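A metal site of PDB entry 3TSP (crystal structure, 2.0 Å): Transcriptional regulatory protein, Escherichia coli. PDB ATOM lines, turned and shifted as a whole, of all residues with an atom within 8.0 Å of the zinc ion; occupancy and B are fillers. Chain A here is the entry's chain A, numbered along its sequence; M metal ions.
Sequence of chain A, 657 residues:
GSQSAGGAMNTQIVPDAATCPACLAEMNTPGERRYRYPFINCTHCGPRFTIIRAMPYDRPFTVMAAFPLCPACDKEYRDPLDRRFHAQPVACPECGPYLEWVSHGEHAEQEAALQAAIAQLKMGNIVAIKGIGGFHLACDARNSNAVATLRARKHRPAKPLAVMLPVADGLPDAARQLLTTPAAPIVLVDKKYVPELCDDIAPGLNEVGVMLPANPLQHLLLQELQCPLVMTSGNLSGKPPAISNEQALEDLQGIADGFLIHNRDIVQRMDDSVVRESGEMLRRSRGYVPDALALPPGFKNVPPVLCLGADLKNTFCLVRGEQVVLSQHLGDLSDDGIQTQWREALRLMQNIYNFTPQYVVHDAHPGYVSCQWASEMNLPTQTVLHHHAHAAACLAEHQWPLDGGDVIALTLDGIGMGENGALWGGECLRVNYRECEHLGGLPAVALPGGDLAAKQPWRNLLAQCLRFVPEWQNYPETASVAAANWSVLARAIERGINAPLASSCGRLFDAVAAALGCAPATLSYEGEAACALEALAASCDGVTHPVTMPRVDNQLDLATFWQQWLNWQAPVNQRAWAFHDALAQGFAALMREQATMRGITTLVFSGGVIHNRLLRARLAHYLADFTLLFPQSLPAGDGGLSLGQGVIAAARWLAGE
SG of Cys 73 lies close to NH2 of Arg 33, 3.3 Å away.
The side-chain sulfur (SG) of Cys 73 lies close to the guanidinium group (NH1) of Arg 34, 3.4 Å away.
The guanidinium group (NE) of Arg 33 lies close to the side-chain sulfur (SG) of Cys 92.
The side-chain sulfur (SG) of Cys 92 lies close to the backbone NH (N) of Glu 94.
The side-chain hydroxyl of Tyr 37 lies within hydrogen-bond range of the backbone carbonyl oxygen of Cys 92 (3.4 Å).
The side-chain sulfur (SG) of Cys 70 lies close to the backbone NH (N) of Ala 72 (3.7 Å).
The zinc ion is bound by SG of Cys 95 (2.2 Å).
SG of Cys 73 binds the zinc ion, 2.2 Å away.
SG of Cys 92 is bound to the zinc ion, at 2.5 Å.
SG of Cys 70 binds the zinc ion, 2.5 Å away.
The zinc ion has four donor atoms within binding distance.
Of the 20 residues printed, 4 come within 4 Å of the zinc ion.
The nearest printed residue that does not touch the zinc ion is Ala 91 (4.3 Å).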
ATOM      1  N   ARG A  33     -16.898   3.534   2.684  1.00  0.00           N
ATOM      2  CA  ARG A  33     -17.578   2.230   2.544  1.00  0.00           C
ATOM      3  C   ARG A  33     -17.487   1.692   1.104  1.00  0.00           C
ATOM      4  O   ARG A  33     -17.524   0.468   0.884  1.00  0.00           O
ATOM      5  CB  ARG A  33     -19.048   2.349   2.974  1.00  0.00           C
ATOM      6  CG  ARG A  33     -19.807   1.009   3.092  1.00  0.00           C
ATOM      7  CD  ARG A  33     -21.234   1.188   3.724  1.00  0.00           C
ATOM      8  NE  ARG A  33     -22.283   1.530   2.758  1.00  0.00           N
ATOM      9  CZ  ARG A  33     -22.663   2.768   2.466  1.00  0.00           C
ATOM     10  NH1 ARG A  33     -22.105   3.804   3.083  1.00  0.00           N
ATOM     11  NH2 ARG A  33     -23.619   2.986   1.574  1.00  0.00           N
ATOM     12  N   ARG A  34     -17.357   2.613   0.140  1.00  0.00           N
ATOM     13  CA  ARG A  34     -17.222   2.247  -1.253  1.00  0.00           C
ATOM     14  C   ARG A  34     -15.793   2.334  -1.778  1.00  0.00           C
ATOM     15  O   ARG A  34     -15.573   2.394  -3.005  1.00  0.00           O
ATOM     16  CB  ARG A  34     -18.156   3.092  -2.111  1.00  0.00           C
ATOM     17  CG  ARG A  34     -19.628   2.791  -1.851  1.00  0.00           C
ATOM     18  CD  ARG A  34     -20.519   3.451  -2.857  1.00  0.00           C
ATOM     19  NE  ARG A  34     -21.913   3.207  -2.553  1.00  0.00           N
ATOM     20  CZ  ARG A  34     -22.657   3.997  -1.776  1.00  0.00           C
ATOM     21  NH1 ARG A  34     -23.930   3.675  -1.546  1.00  0.00           N
ATOM     22  NH2 ARG A  34     -22.137   5.096  -1.236  1.00  0.00           N
ATOM     23  N   TYR A  37     -14.709  -0.089  -4.470  1.00  0.00           N
ATOM     24  CA  TYR A  37     -15.892  -0.803  -4.934  1.00  0.00           C
ATOM     25  C   TYR A  37     -16.102  -0.628  -6.455  1.00  0.00           C
ATOM     26  O   TYR A  37     -16.360   0.481  -6.912  1.00  0.00           O
ATOM     27  CB  TYR A  37     -17.147  -0.353  -4.195  1.00  0.00           C
ATOM     28  CG  TYR A  37     -18.327  -1.220  -4.513  1.00  0.00           C
ATOM     29  CD1 TYR A  37     -18.194  -2.611  -4.450  1.00  0.00           C
ATOM     30  CD2 TYR A  37     -19.548  -0.676  -4.894  1.00  0.00           C
ATOM     31  CE1 TYR A  37     -19.240  -3.430  -4.718  1.00  0.00           C
ATOM     32  CE2 TYR A  37     -20.628  -1.512  -5.182  1.00  0.00           C
ATOM     33  CZ  TYR A  37     -20.454  -2.884  -5.080  1.00  0.00           C
ATOM     34  OH  TYR A  37     -21.468  -3.778  -5.364  1.00  0.00           O
ATOM     35  N   ARG A  59     -35.555   0.978  -9.451  1.00  0.00           N
ATOM     36  CA  ARG A  59     -34.747  -0.181  -9.110  1.00  0.00           C
ATOM     37  C   ARG A  59     -35.429  -1.558  -9.370  1.00  0.00           C
ATOM     38  O   ARG A  59     -34.775  -2.457  -9.932  1.00  0.00           O
ATOM     39  CB  ARG A  59     -34.189  -0.061  -7.686  1.00  0.00           C
ATOM     40  CG  ARG A  59     -33.160  -1.103  -7.316  1.00  0.00           C
ATOM     41  CD  ARG A  59     -32.576  -0.845  -5.920  1.00  0.00           C
ATOM     42  NE  ARG A  59     -31.569  -1.841  -5.558  1.00  0.00           N
ATOM     43  CZ  ARG A  59     -30.244  -1.651  -5.648  1.00  0.00           C
ATOM     44  NH1 ARG A  59     -29.745  -0.499  -6.092  1.00  0.00           N
ATOM     45  NH2 ARG A  59     -29.404  -2.620  -5.288  1.00  0.00           N
ATOM     46  N   PHE A  67     -30.612  -7.240  -5.708  1.00  0.00           N
ATOM     47  CA  PHE A  67     -29.645  -6.843  -4.693  1.00  0.00           C
ATOM     48  C   PHE A  67     -30.263  -5.894  -3.662  1.00  0.00           C
ATOM     49  O   PHE A  67     -30.052  -4.687  -3.737  1.00  0.00           O
ATOM     50  CB  PHE A  67     -28.454  -6.121  -5.355  1.00  0.00           C
ATOM     51  CG  PHE A  67     -27.646  -6.980  -6.273  1.00  0.00           C
ATOM     52  CD1 PHE A  67     -26.632  -7.801  -5.778  1.00  0.00           C
ATOM     53  CD2 PHE A  67     -27.885  -6.973  -7.658  1.00  0.00           C
ATOM     54  CE1 PHE A  67     -25.863  -8.596  -6.646  1.00  0.00           C
ATOM     55  CE2 PHE A  67     -27.125  -7.771  -8.523  1.00  0.00           C
ATOM     56  CZ  PHE A  67     -26.107  -8.580  -8.009  1.00  0.00           C
ATOM     57  N   PRO A  68     -30.975  -6.424  -2.659  1.00  0.00           N
ATOM     58  CA  PRO A  68     -31.597  -5.496  -1.688  1.00  0.00           C
ATOM     59  C   PRO A  68     -30.566  -4.607  -0.990  1.00  0.00           C
ATOM     60  O   PRO A  68     -29.538  -5.099  -0.510  1.00  0.00           O
ATOM     61  CB  PRO A  68     -32.297  -6.432  -0.672  1.00  0.00           C
ATOM     62  CG  PRO A  68     -32.457  -7.754  -1.434  1.00  0.00           C
ATOM     63  CD  PRO A  68     -31.259  -7.839  -2.348  1.00  0.00           C
ATOM     64  N   LEU A  69     -30.826  -3.313  -0.944  1.00  0.00           N
ATOM     65  CA  LEU A  69     -29.886  -2.362  -0.358  1.00  0.00           C
ATOM     66  C   LEU A  69     -29.651  -2.685   1.113  1.00  0.00           C
ATOM     67  O   LEU A  69     -30.579  -3.098   1.788  1.00  0.00           O
ATOM     68  CB  LEU A  69     -30.381  -0.933  -0.521  1.00  0.00           C
ATOM     69  CG  LEU A  69     -30.397  -0.401  -1.948  1.00  0.00           C
ATOM     70  CD1 LEU A  69     -30.875   1.012  -1.938  1.00  0.00           C
ATOM     71  CD2 LEU A  69     -29.022  -0.499  -2.591  1.00  0.00           C
ATOM     72  N   CYS A  70     -28.428  -2.493   1.601  1.00  0.00           N
ATOM     73  CA  CYS A  70     -28.137  -2.540   3.056  1.00  0.00           C
ATOM     74  C   CYS A  70     -28.717  -1.248   3.663  1.00  0.00           C
ATOM     75  O   CYS A  70     -29.149  -0.370   2.919  1.00  0.00           O
ATOM     76  CB  CYS A  70     -26.625  -2.637   3.295  1.00  0.00           C
ATOM     77  SG  CYS A  70     -25.732  -1.097   2.890  1.00  0.00           S
ATOM     78  N   PRO A  71     -28.750  -1.126   5.019  1.00  0.00           N
ATOM     79  CA  PRO A  71     -29.292   0.123   5.586  1.00  0.00           C
ATOM     80  C   PRO A  71     -28.554   1.426   5.214  1.00  0.00           C
ATOM     81  O   PRO A  71     -29.213   2.433   4.973  1.00  0.00           O
ATOM     82  CB  PRO A  71     -29.265  -0.151   7.108  1.00  0.00           C
ATOM     83  CG  PRO A  71     -29.318  -1.673   7.207  1.00  0.00           C
ATOM     84  CD  PRO A  71     -28.419  -2.095   6.085  1.00  0.00           C
ATOM     85  N   ALA A  72     -27.216   1.425   5.144  1.00  0.00           N
ATOM     86  CA  ALA A  72     -26.484   2.677   4.819  1.00  0.00           C
ATOM     87  C   ALA A  72     -26.757   3.135   3.383  1.00  0.00           C
ATOM     88  O   ALA A  72     -27.010   4.318   3.150  1.00  0.00           O
ATOM     89  CB  ALA A  72     -24.987   2.526   5.077  1.00  0.00           C
ATOM     90  N   CYS A  73     -26.724   2.189   2.429  1.00  0.00           N
ATOM     91  CA  CYS A  73     -27.142   2.454   1.051  1.00  0.00           C
ATOM     92  C   CYS A  73     -28.572   2.966   0.927  1.00  0.00           C
ATOM     93  O   CYS A  73     -28.851   3.886   0.153  1.00  0.00           O
ATOM     94  CB  CYS A  73     -27.004   1.193   0.223  1.00  0.00           C
ATOM     95  SG  CYS A  73     -25.295   0.868  -0.257  1.00  0.00           S
ATOM     96  N   ASP A  74     -29.465   2.347   1.678  1.00  0.00           N
ATOM     97  CA  ASP A  74     -30.877   2.700   1.611  1.00  0.00           C
ATOM     98  C   ASP A  74     -31.131   4.140   2.096  1.00  0.00           C
ATOM     99  O   ASP A  74     -31.893   4.890   1.474  1.00  0.00           O
ATOM    100  CB  ASP A  74     -31.688   1.649   2.377  1.00  0.00           C
ATOM    101  CG  ASP A  74     -33.192   1.860   2.265  1.00  0.00           C
ATOM    102  OD1 ASP A  74     -33.743   1.783   1.151  1.00  0.00           O
ATOM    103  OD2 ASP A  74     -33.804   2.096   3.332  1.00  0.00           O
ATOM    104  N   GLU A  76     -28.968   6.636   1.912  1.00  0.00           N
ATOM    105  CA  GLU A  76     -28.441   7.546   0.909  1.00  0.00           C
ATOM    106  C   GLU A  76     -29.386   7.664  -0.305  1.00  0.00           C
ATOM    107  O   GLU A  76     -29.639   8.784  -0.807  1.00  0.00           O
ATOM    108  CB  GLU A  76     -27.033   7.130   0.467  1.00  0.00           C
ATOM    109  CG  GLU A  76     -25.986   7.247   1.581  1.00  0.00           C
ATOM    110  CD  GLU A  76     -24.733   6.411   1.289  1.00  0.00           C
ATOM    111  OE1 GLU A  76     -24.606   5.881   0.162  1.00  0.00           O
ATOM    112  OE2 GLU A  76     -23.888   6.282   2.189  1.00  0.00           O
ATOM    113  N   VAL A  90     -27.702   1.896  -7.397  1.00  0.00           N
ATOM    114  CA  VAL A  90     -26.754   2.146  -6.303  1.00  0.00           C
ATOM    115  C   VAL A  90     -26.421   0.839  -5.572  1.00  0.00           C
ATOM    116  O   VAL A  90     -27.253  -0.077  -5.513  1.00  0.00           O
ATOM    117  CB  VAL A  90     -27.282   3.236  -5.299  1.00  0.00           C
ATOM    118  CG1 VAL A  90     -28.549   2.775  -4.579  1.00  0.00           C
ATOM    119  CG2 VAL A  90     -26.197   3.647  -4.280  1.00  0.00           C
ATOM    120  N   ALA A  91     -25.216   0.742  -5.028  1.00  0.00           N
ATOM    121  CA  ALA A  91     -24.792  -0.372  -4.192  1.00  0.00           C
ATOM    122  C   ALA A  91     -23.508  -0.054  -3.407  1.00  0.00           C
ATOM    123  O   ALA A  91     -22.884   0.992  -3.600  1.00  0.00           O
ATOM    124  CB  ALA A  91     -24.580  -1.598  -5.067  1.00  0.00           C
ATOM    125  N   CYS A  92     -23.107  -0.979  -2.525  1.00  0.00           N
ATOM    126  CA  CYS A  92     -21.789  -0.930  -1.868  1.00  0.00           C
ATOM    127  C   CYS A  92     -21.288  -2.368  -1.758  1.00  0.00           C
ATOM    128  O   CYS A  92     -22.048  -3.281  -2.099  1.00  0.00           O
ATOM    129  CB  CYS A  92     -21.882  -0.280  -0.498  1.00  0.00           C
ATOM    130  SG  CYS A  92     -22.470  -1.365   0.830  1.00  0.00           S
ATOM    131  N   PRO A  93     -20.046  -2.580  -1.270  1.00  0.00           N
ATOM    132  CA  PRO A  93     -19.530  -3.954  -1.138  1.00  0.00           C
ATOM    133  C   PRO A  93     -20.421  -4.920  -0.301  1.00  0.00           C
ATOM    134  O   PRO A  93     -20.426  -6.137  -0.552  1.00  0.00           O
ATOM    135  CB  PRO A  93     -18.165  -3.742  -0.466  1.00  0.00           C
ATOM    136  CG  PRO A  93     -17.760  -2.354  -0.918  1.00  0.00           C
ATOM    137  CD  PRO A  93     -19.037  -1.595  -0.813  1.00  0.00           C
ATOM    138  N   GLU A  94     -21.159  -4.373   0.669  1.00  0.00           N
ATOM    139  CA  GLU A  94     -22.028  -5.181   1.541  1.00  0.00           C
ATOM    140  C   GLU A  94     -23.208  -5.784   0.795  1.00  0.00           C
ATOM    141  O   GLU A  94     -23.548  -6.955   0.992  1.00  0.00           O
ATOM    142  CB  GLU A  94     -22.563  -4.316   2.709  1.00  0.00           C
ATOM    143  CG  GLU A  94     -21.899  -4.552   4.072  1.00  0.00           C
ATOM    144  CD  GLU A  94     -20.391  -4.834   3.988  1.00  0.00           C
ATOM    145  OE1 GLU A  94     -19.983  -5.964   4.368  1.00  0.00           O
ATOM    146  OE2 GLU A  94     -19.618  -3.932   3.538  1.00  0.00           O
ATOM    147  N   CYS A  95     -23.844  -4.979  -0.059  1.00  0.00           N
ATOM    148  CA  CYS A  95     -25.125  -5.367  -0.651  1.00  0.00           C
ATOM    149  C   CYS A  95     -25.130  -5.466  -2.175  1.00  0.00           C
ATOM    150  O   CYS A  95     -26.150  -5.811  -2.757  1.00  0.00           O
ATOM    151  CB  CYS A  95     -26.240  -4.400  -0.211  1.00  0.00           C
ATOM    152  SG  CYS A  95     -25.908  -2.700  -0.693  1.00  0.00           S
ATOM    153  N   GLY A  96     -24.013  -5.158  -2.828  1.00  0.00           N
ATOM    154  CA  GLY A  96     -24.003  -5.131  -4.292  1.00  0.00           C
ATOM    155  C   GLY A  96     -23.335  -6.314  -4.987  1.00  0.00           C
ATOM    156  O   GLY A  96     -22.954  -7.315  -4.313  1.00  0.00           O
HETATM  157 ZN    ZN M   1     -24.893  -1.180   0.513  1.00  0.00          ZN
